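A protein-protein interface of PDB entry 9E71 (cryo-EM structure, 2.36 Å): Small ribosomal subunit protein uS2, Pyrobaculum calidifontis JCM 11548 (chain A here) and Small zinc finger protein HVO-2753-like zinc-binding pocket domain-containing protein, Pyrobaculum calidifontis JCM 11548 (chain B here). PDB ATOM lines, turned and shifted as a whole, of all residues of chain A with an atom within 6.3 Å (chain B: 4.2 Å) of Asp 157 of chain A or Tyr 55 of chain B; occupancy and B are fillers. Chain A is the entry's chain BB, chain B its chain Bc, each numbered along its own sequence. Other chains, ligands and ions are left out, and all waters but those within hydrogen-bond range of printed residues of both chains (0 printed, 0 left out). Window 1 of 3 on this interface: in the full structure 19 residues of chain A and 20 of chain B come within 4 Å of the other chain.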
ATOM      1  N   ARG A  35      10.143  -6.236 -27.629  1.00  0.00           N
ATOM      2  CA  ARG A  35      11.414  -5.876 -27.011  1.00  0.00           C
ATOM      3  C   ARG A  35      11.745  -6.785 -25.839  1.00  0.00           C
ATOM      4  O   ARG A  35      12.922  -7.046 -25.568  1.00  0.00           O
ATOM      5  CB  ARG A  35      11.380  -4.428 -26.545  1.00  0.00           C
ATOM      6  CG  ARG A  35      11.098  -3.434 -27.641  1.00  0.00           C
ATOM      7  CD  ARG A  35      11.878  -3.773 -28.878  1.00  0.00           C
ATOM      8  NE  ARG A  35      13.113  -3.009 -28.949  1.00  0.00           N
ATOM      9  CZ  ARG A  35      13.797  -2.800 -30.064  1.00  0.00           C
ATOM     10  NH1 ARG A  35      13.355  -3.223 -31.237  1.00  0.00           N
ATOM     11  NH2 ARG A  35      14.950  -2.148 -30.002  1.00  0.00           N
ATOM     12  N   LEU A  64      24.524   6.953 -19.522  1.00  0.00           N
ATOM     13  CA  LEU A  64      24.226   7.893 -20.598  1.00  0.00           C
ATOM     14  C   LEU A  64      24.227   9.338 -20.103  1.00  0.00           C
ATOM     15  O   LEU A  64      24.883  10.203 -20.695  1.00  0.00           O
ATOM     16  CB  LEU A  64      22.886   7.546 -21.241  1.00  0.00           C
ATOM     17  CG  LEU A  64      22.555   8.352 -22.495  1.00  0.00           C
ATOM     18  CD1 LEU A  64      23.810   8.610 -23.317  1.00  0.00           C
ATOM     19  CD2 LEU A  64      21.516   7.633 -23.322  1.00  0.00           C
ATOM     20  N   ILE A 141      17.342  16.427 -30.809  1.00  0.00           N
ATOM     21  CA  ILE A 141      17.918  16.314 -29.477  1.00  0.00           C
ATOM     22  C   ILE A 141      17.632  14.907 -28.977  1.00  0.00           C
ATOM     23  O   ILE A 141      16.508  14.429 -29.125  1.00  0.00           O
ATOM     24  CB  ILE A 141      17.343  17.353 -28.498  1.00  0.00           C
ATOM     25  CG1 ILE A 141      17.558  18.768 -29.030  1.00  0.00           C
ATOM     26  CG2 ILE A 141      17.962  17.184 -27.127  1.00  0.00           C
ATOM     27  CD1 ILE A 141      19.019  19.156 -29.190  1.00  0.00           C
ATOM     28  N   PRO A 142      18.614  14.203 -28.418  1.00  0.00           N
ATOM     29  CA  PRO A 142      18.350  12.863 -27.878  1.00  0.00           C
ATOM     30  C   PRO A 142      17.356  12.901 -26.726  1.00  0.00           C
ATOM     31  O   PRO A 142      17.309  13.855 -25.948  1.00  0.00           O
ATOM     32  CB  PRO A 142      19.726  12.377 -27.410  1.00  0.00           C
ATOM     33  CG  PRO A 142      20.688  13.472 -27.688  1.00  0.00           C
ATOM     34  CD  PRO A 142      20.045  14.527 -28.496  1.00  0.00           C
ATOM     35  N   VAL A 143      16.548  11.847 -26.631  1.00  0.00           N
ATOM     36  CA  VAL A 143      15.423  11.796 -25.706  1.00  0.00           C
ATOM     37  C   VAL A 143      15.480  10.504 -24.906  1.00  0.00           C
ATOM     38  O   VAL A 143      15.714   9.428 -25.468  1.00  0.00           O
ATOM     39  CB  VAL A 143      14.076  11.906 -26.441  1.00  0.00           C
ATOM     40  CG1 VAL A 143      12.923  11.712 -25.466  1.00  0.00           C
ATOM     41  CG2 VAL A 143      13.978  13.245 -27.143  1.00  0.00           C
ATOM     42  N   VAL A 144      15.261  10.616 -23.600  1.00  0.00           N
ATOM     43  CA  VAL A 144      15.144   9.480 -22.698  1.00  0.00           C
ATOM     44  C   VAL A 144      13.794   9.572 -22.004  1.00  0.00           C
ATOM     45  O   VAL A 144      13.327  10.671 -21.683  1.00  0.00           O
ATOM     46  CB  VAL A 144      16.286   9.450 -21.665  1.00  0.00           C
ATOM     47  CG1 VAL A 144      16.288   8.128 -20.916  1.00  0.00           C
ATOM     48  CG2 VAL A 144      17.616   9.696 -22.349  1.00  0.00           C
ATOM     49  N   HIS A 153       6.066   5.230 -28.376  1.00  0.00           N
ATOM     50  CA  HIS A 153       7.509   5.062 -28.419  1.00  0.00           C
ATOM     51  C   HIS A 153       8.180   5.903 -29.494  1.00  0.00           C
ATOM     52  O   HIS A 153       9.387   5.759 -29.708  1.00  0.00           O
ATOM     53  CB  HIS A 153       7.853   3.592 -28.644  1.00  0.00           C
ATOM     54  CG  HIS A 153       7.252   3.028 -29.889  1.00  0.00           C
ATOM     55  ND1 HIS A 153       6.021   2.414 -29.905  1.00  0.00           N
ATOM     56  CD2 HIS A 153       7.697   3.015 -31.167  1.00  0.00           C
ATOM     57  CE1 HIS A 153       5.740   2.028 -31.136  1.00  0.00           C
ATOM     58  NE2 HIS A 153       6.740   2.383 -31.922  1.00  0.00           N
ATOM     59  N   TYR A 155      10.115   8.707 -31.421  1.00  0.00           N
ATOM     60  CA  TYR A 155      11.116   9.731 -31.132  1.00  0.00           C
ATOM     61  C   TYR A 155      11.793   9.554 -29.782  1.00  0.00           C
ATOM     62  O   TYR A 155      12.317  10.520 -29.226  1.00  0.00           O
ATOM     63  CB  TYR A 155      10.507  11.129 -31.203  1.00  0.00           C
ATOM     64  CG  TYR A 155       9.936  11.470 -32.546  1.00  0.00           C
ATOM     65  CD1 TYR A 155      10.646  11.218 -33.703  1.00  0.00           C
ATOM     66  CD2 TYR A 155       8.689  12.054 -32.655  1.00  0.00           C
ATOM     67  CE1 TYR A 155      10.127  11.538 -34.933  1.00  0.00           C
ATOM     68  CE2 TYR A 155       8.166  12.385 -33.879  1.00  0.00           C
ATOM     69  CZ  TYR A 155       8.882  12.115 -35.016  1.00  0.00           C
ATOM     70  OH  TYR A 155       8.350  12.435 -36.243  1.00  0.00           O
ATOM     71  N   ILE A 156      11.803   8.350 -29.229  1.00  0.00           N
ATOM     72  CA  ILE A 156      12.473   8.092 -27.962  1.00  0.00           C
ATOM     73  C   ILE A 156      13.738   7.305 -28.261  1.00  0.00           C
ATOM     74  O   ILE A 156      13.678   6.136 -28.651  1.00  0.00           O
ATOM     75  CB  ILE A 156      11.569   7.345 -26.978  1.00  0.00           C
ATOM     76  CG1 ILE A 156      10.240   8.078 -26.840  1.00  0.00           C
ATOM     77  CG2 ILE A 156      12.245   7.241 -25.631  1.00  0.00           C
ATOM     78  CD1 ILE A 156      10.208   9.049 -25.705  1.00  0.00           C
ATOM     79  N   ASP A 157      14.885   7.954 -28.080  1.00  0.00           N
ATOM     80  CA  ASP A 157      16.176   7.329 -28.318  1.00  0.00           C
ATOM     81  C   ASP A 157      16.581   6.380 -27.206  1.00  0.00           C
ATOM     82  O   ASP A 157      17.380   5.472 -27.449  1.00  0.00           O
ATOM     83  CB  ASP A 157      17.236   8.408 -28.488  1.00  0.00           C
ATOM     84  CG  ASP A 157      16.737   9.574 -29.302  1.00  0.00           C
ATOM     85  OD1 ASP A 157      16.504   9.397 -30.511  1.00  0.00           O
ATOM     86  OD2 ASP A 157      16.527  10.659 -28.731  1.00  0.00           O
ATOM     87  N   PHE A 158      16.069   6.574 -25.995  1.00  0.00           N
ATOM     88  CA  PHE A 158      16.314   5.629 -24.920  1.00  0.00           C
ATOM     89  C   PHE A 158      15.090   5.567 -24.021  1.00  0.00           C
ATOM     90  O   PHE A 158      14.515   6.600 -23.663  1.00  0.00           O
ATOM     91  CB  PHE A 158      17.554   6.009 -24.112  1.00  0.00           C
ATOM     92  CG  PHE A 158      18.040   4.920 -23.209  1.00  0.00           C
ATOM     93  CD1 PHE A 158      18.821   3.892 -23.704  1.00  0.00           C
ATOM     94  CD2 PHE A 158      17.716   4.921 -21.866  1.00  0.00           C
ATOM     95  CE1 PHE A 158      19.270   2.886 -22.876  1.00  0.00           C
ATOM     96  CE2 PHE A 158      18.164   3.918 -21.034  1.00  0.00           C
ATOM     97  CZ  PHE A 158      18.943   2.900 -21.540  1.00  0.00           C
ATOM     98  N   MET A 159      14.698   4.349 -23.660  1.00  0.00           N
ATOM     99  CA  MET A 159      13.510   4.128 -22.855  1.00  0.00           C
ATOM    100  C   MET A 159      13.835   3.216 -21.686  1.00  0.00           C
ATOM    101  O   MET A 159      14.642   2.291 -21.810  1.00  0.00           O
ATOM    102  CB  MET A 159      12.379   3.513 -23.679  1.00  0.00           C
ATOM    103  CG  MET A 159      12.810   2.363 -24.564  1.00  0.00           C
ATOM    104  SD  MET A 159      11.772   2.229 -26.026  1.00  0.00           S
ATOM    105  CE  MET A 159      10.604   0.991 -25.480  1.00  0.00           C
ATOM    106  N   PHE B  32      24.553  10.295 -31.269  1.00  0.00           N
ATOM    107  CA  PHE B  32      25.057  10.235 -29.901  1.00  0.00           C
ATOM    108  C   PHE B  32      26.052   9.086 -29.811  1.00  0.00           C
ATOM    109  O   PHE B  32      26.439   8.497 -30.820  1.00  0.00           O
ATOM    110  CB  PHE B  32      23.911  10.120 -28.882  1.00  0.00           C
ATOM    111  CG  PHE B  32      22.909   9.033 -29.183  1.00  0.00           C
ATOM    112  CD1 PHE B  32      21.812   9.282 -29.981  1.00  0.00           C
ATOM    113  CD2 PHE B  32      23.047   7.775 -28.633  1.00  0.00           C
ATOM    114  CE1 PHE B  32      20.890   8.293 -30.243  1.00  0.00           C
ATOM    115  CE2 PHE B  32      22.130   6.783 -28.893  1.00  0.00           C
ATOM    116  CZ  PHE B  32      21.052   7.040 -29.699  1.00  0.00           C
ATOM    117  N   ILE B  42      26.140   6.265 -32.563  1.00  0.00           N
ATOM    118  CA  ILE B  42      24.826   5.820 -33.001  1.00  0.00           C
ATOM    119  C   ILE B  42      24.159   6.988 -33.709  1.00  0.00           C
ATOM    120  O   ILE B  42      24.024   8.078 -33.137  1.00  0.00           O
ATOM    121  CB  ILE B  42      23.972   5.323 -31.827  1.00  0.00           C
ATOM    122  CG1 ILE B  42      24.652   4.135 -31.153  1.00  0.00           C
ATOM    123  CG2 ILE B  42      22.586   4.946 -32.305  1.00  0.00           C
ATOM    124  CD1 ILE B  42      24.887   2.977 -32.082  1.00  0.00           C
ATOM    125  N   ARG B  44      20.698   8.118 -35.829  1.00  0.00           N
ATOM    126  CA  ARG B  44      19.303   7.811 -36.104  1.00  0.00           C
ATOM    127  C   ARG B  44      18.713   8.938 -36.930  1.00  0.00           C
ATOM    128  O   ARG B  44      18.618  10.072 -36.453  1.00  0.00           O
ATOM    129  CB  ARG B  44      18.508   7.631 -34.809  1.00  0.00           C
ATOM    130  CG  ARG B  44      18.546   6.230 -34.255  1.00  0.00           C
ATOM    131  CD  ARG B  44      18.215   6.203 -32.778  1.00  0.00           C
ATOM    132  NE  ARG B  44      16.779   6.200 -32.511  1.00  0.00           N
ATOM    133  CZ  ARG B  44      15.949   5.205 -32.802  1.00  0.00           C
ATOM    134  NH1 ARG B  44      16.361   4.118 -33.431  1.00  0.00           N
ATOM    135  NH2 ARG B  44      14.672   5.303 -32.448  1.00  0.00           N
ATOM    136  N   ARG B  49      13.825   7.335 -36.011  1.00  0.00           N
ATOM    137  CA  ARG B  49      13.404   7.790 -34.689  1.00  0.00           C
ATOM    138  C   ARG B  49      11.892   7.714 -34.538  1.00  0.00           C
ATOM    139  O   ARG B  49      11.382   7.266 -33.505  1.00  0.00           O
ATOM    140  CB  ARG B  49      13.910   9.211 -34.432  1.00  0.00           C
ATOM    141  CG  ARG B  49      15.403   9.360 -34.636  1.00  0.00           C
ATOM    142  CD  ARG B  49      15.856  10.807 -34.780  1.00  0.00           C
ATOM    143  NE  ARG B  49      15.109  11.747 -33.956  1.00  0.00           N
ATOM    144  CZ  ARG B  49      15.260  11.869 -32.646  1.00  0.00           C
ATOM    145  NH1 ARG B  49      16.062  11.069 -31.972  1.00  0.00           N
ATOM    146  NH2 ARG B  49      14.593  12.817 -32.001  1.00  0.00           N
ATOM    147  N   VAL B  53      12.921   2.269 -34.991  1.00  0.00           N
ATOM    148  CA  VAL B  53      13.774   1.227 -35.555  1.00  0.00           C
ATOM    149  C   VAL B  53      14.906   0.920 -34.584  1.00  0.00           C
ATOM    150  O   VAL B  53      15.598   1.839 -34.130  1.00  0.00           O
ATOM    151  CB  VAL B  53      14.324   1.642 -36.926  1.00  0.00           C
ATOM    152  CG1 VAL B  53      15.436   0.707 -37.347  1.00  0.00           C
ATOM    153  CG2 VAL B  53      13.215   1.648 -37.953  1.00  0.00           C
ATOM    154  N   PRO B  54      15.136  -0.345 -34.250  1.00  0.00           N
ATOM    155  CA  PRO B  54      16.188  -0.674 -33.287  1.00  0.00           C
ATOM    156  C   PRO B  54      17.573  -0.459 -33.867  1.00  0.00           C
ATOM    157  O   PRO B  54      17.776  -0.471 -35.083  1.00  0.00           O
ATOM    158  CB  PRO B  54      15.948  -2.153 -32.977  1.00  0.00           C
ATOM    159  CG  PRO B  54      15.027  -2.662 -34.035  1.00  0.00           C
ATOM    160  CD  PRO B  54      14.561  -1.536 -34.892  1.00  0.00           C
ATOM    161  N   TYR B  55      18.533  -0.250 -32.971  1.00  0.00           N
ATOM    162  CA  TYR B  55      19.930  -0.081 -33.335  1.00  0.00           C
ATOM    163  C   TYR B  55      20.795  -0.987 -32.473  1.00  0.00           C
ATOM    164  O   TYR B  55      20.477  -1.252 -31.312  1.00  0.00           O
ATOM    165  CB  TYR B  55      20.374   1.378 -33.186  1.00  0.00           C
ATOM    166  CG  TYR B  55      20.039   2.014 -31.855  1.00  0.00           C
ATOM    167  CD1 TYR B  55      20.874   1.866 -30.755  1.00  0.00           C
ATOM    168  CD2 TYR B  55      18.887   2.771 -31.701  1.00  0.00           C
ATOM    169  CE1 TYR B  55      20.571   2.448 -29.546  1.00  0.00           C
ATOM    170  CE2 TYR B  55      18.579   3.359 -30.495  1.00  0.00           C
ATOM    171  CZ  TYR B  55      19.426   3.195 -29.422  1.00  0.00           C
ATOM    172  OH  TYR B  55      19.132   3.774 -28.213  1.00  0.00           O
ATOM    173  N   ARG B  56      21.904  -1.440 -33.044  1.00  0.00           N
ATOM    174  CA  ARG B  56      22.793  -2.384 -32.387  1.00  0.00           C
ATOM    175  C   ARG B  56      24.198  -1.807 -32.333  1.00  0.00           C
ATOM    176  O   ARG B  56      24.651  -1.170 -33.289  1.00  0.00           O
ATOM    177  CB  ARG B  56      22.802  -3.725 -33.127  1.00  0.00           C
ATOM    178  CG  ARG B  56      22.463  -4.908 -32.258  1.00  0.00           C
ATOM    179  CD  ARG B  56      22.785  -6.224 -32.949  1.00  0.00           C
ATOM    180  NE  ARG B  56      24.182  -6.627 -32.842  1.00  0.00           N
ATOM    181  CZ  ARG B  56      24.821  -6.871 -31.705  1.00  0.00           C
ATOM    182  NH1 ARG B  56      24.198  -6.840 -30.539  1.00  0.00           N
ATOM    183  NH2 ARG B  56      26.113  -7.185 -31.742  1.00  0.00           N
ATOM    184  N   PHE B  62      24.192  -4.343 -27.312  1.00  0.00           N
ATOM    185  CA  PHE B  62      23.087  -3.552 -26.787  1.00  0.00           C
ATOM    186  C   PHE B  62      22.195  -3.083 -27.926  1.00  0.00           C
ATOM    187  O   PHE B  62      22.681  -2.502 -28.903  1.00  0.00           O
ATOM    188  CB  PHE B  62      23.597  -2.350 -25.992  1.00  0.00           C
ATOM    189  CG  PHE B  62      22.545  -1.324 -25.682  1.00  0.00           C
ATOM    190  CD1 PHE B  62      21.636  -1.535 -24.663  1.00  0.00           C
ATOM    191  CD2 PHE B  62      22.487  -0.134 -26.385  1.00  0.00           C
ATOM    192  CE1 PHE B  62      20.678  -0.593 -24.369  1.00  0.00           C
ATOM    193  CE2 PHE B  62      21.528   0.811 -26.095  1.00  0.00           C
ATOM    194  CZ  PHE B  62      20.624   0.581 -25.084  1.00  0.00           C
ATOM    195  N   VAL B  63      20.895  -3.320 -27.783  1.00  0.00           N
ATOM    196  CA  VAL B  63      19.888  -2.870 -28.736  1.00  0.00           C
ATOM    197  C   VAL B  63      19.006  -1.846 -28.042  1.00  0.00           C
ATOM    198  O   VAL B  63      18.375  -2.153 -27.023  1.00  0.00           O
ATOM    199  CB  VAL B  63      19.044  -4.043 -29.263  1.00  0.00           C
ATOM    200  CG1 VAL B  63      19.788  -4.789 -30.345  1.00  0.00           C
ATOM    201  CG2 VAL B  63      18.666  -4.978 -28.128  1.00  0.00           C
ATOM    202  N   GLY B  64      19.013  -0.618 -28.553  1.00  0.00           N
ATOM    203  CA  GLY B  64      18.254   0.447 -27.876  1.00  0.00           C
ATOM    204  C   GLY B  64      17.140   0.995 -28.740  1.00  0.00           C
ATOM    205  O   GLY B  64      17.053   0.609 -29.922  1.00  0.00           O
ATOM    206  N   PRO B  65      16.276   1.878 -28.201  1.00  0.00           N
ATOM    207  CA  PRO B  65      15.140   2.396 -28.951  1.00  0.00           C
ATOM    208  C   PRO B  65      15.480   2.652 -30.420  1.00  0.00           C
ATOM    209  O   PRO B  65      14.739   2.145 -31.235  1.00  0.00           O
ATOM    210  CB  PRO B  65      14.880   3.694 -28.198  1.00  0.00           C
ATOM    211  CG  PRO B  65      15.116   3.297 -26.769  1.00  0.00           C
ATOM    212  CD  PRO B  65      16.331   2.395 -26.833  1.00  0.00           C
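Of the 12 printed residues of chain B, 7 touch a printed residue of chain A.
Hydrophobic or aromatic side chains of chain B within 4 Å of the printed part of chain A: Pro 54, Tyr 55, Phe 62 and Pro 65.
Along chain B the printed residues that touch a printed residue of chain A span positions 44 to 65.
Among the printed residues, 12 pairs touch across the chains.
Among the printed residues, Asp or Glu carboxylates within 4 Å of a Lys or Arg side-chain nitrogen of the other chain: Asp 157 of chain A with Arg 44 of chain B and Asp 157 of chain A with Arg 49 of chain B.
Leu 64 of chain A touches none of the printed residues of chain B.
Of chain B, only Arg 44, Arg 49, Tyr 55 and Pro 65 come within 4 Å of Asp 157 of chain A.
Phe 32 of chain B touches none of the printed residues of chain A.
Printed residues of chain A within 4 Å of Arg 49 of chain B: Ile 141 (3.8 Å), Tyr 155 (2.8 Å) and Asp 157 (2.3 Å).
Of the printed residues of chain A, Pro 54 of chain B touches Arg 35 (3.1 Å).
Of chain A, only Asp 157 (2.6 Å) comes within 4 Å of Tyr 55 of chain B.
Printed residues of chain A within 4 Å of Gly 64 of chain B: Arg 35.
Printed residues of chain A within 4 Å of Pro 65 of chain B: Ile 156 (2.8 Å), Asp 157 (3.2 Å), Phe 158 (3.2 Å) and Met 159 (3.3 Å).
The nearest printed residue of chain B that does not touch Ile 141 of chain A is Phe 32 of chain B (7.1 Å).
N of Val 143 of chain A sits at hydrogen-bond distance from OD2 of Asp 157 of chain A.
The guanidinium group (NH1) of Arg 44 of chain B is in hydrogen-bond range of the backbone carbonyl oxygen (O) of Val 53 of chain B.
The backbone carbonyl oxygen (O) of Val 143 of chain A lies within hydrogen-bond range of the backbone NH (N) of Phe 158 of chain A, at 2.9 Å.
The guanidinium group of Arg 44 of chain B lies within hydrogen-bond range of the backbone carbonyl oxygen of Pro 65 of chain B (3.4 Å).
N of Gly 64 of chain B lies within hydrogen-bond range of O of Tyr 55 of chain B, at 3.2 Å.
Arg 35 of chain A touches Pro 54 of chain B (NH2 to CB, 3.1 Å).
Ile 141 of chain A touches Arg 49 of chain B (O to NH2, 3.8 Å).
Ile 156 of chain A touches Pro 65 of chain B.
Pro 65 of chain B touches Asp 157 of chain A (CB to O, 3.2 Å).
Phe 62 of chain B touches Phe 158 of chain A.
Phe 158 of chain A touches Pro 65 of chain B.
Met 159 of chain A touches Pro 65 of chain B (N to CG, 3.3 Å).
The backbone carbonyl oxygen (O) of Asp 157 of chain A is in hydrogen-bond range of the side-chain hydroxyl (OH) of Tyr 55 of chain B (2.6 Å).
The backbone NH (N) of Tyr 155 of chain A sits at hydrogen-bond distance from the backbone carbonyl oxygen (O) of Arg 49 of chain B.
NE of Arg 44 of chain B is in salt-bridge range of OD1 of Asp 157 of chain A, 3.8 Å away.
The guanidinium group of Arg 35 of chain A lies within hydrogen-bond range of the backbone carbonyl oxygen of Gly 64 of chain B (3.5 Å).
The side-chain carboxylate of Asp 157 of chain A lies within salt-bridge range of the guanidinium group of Arg 49 of chain B, 3.3 Å away.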
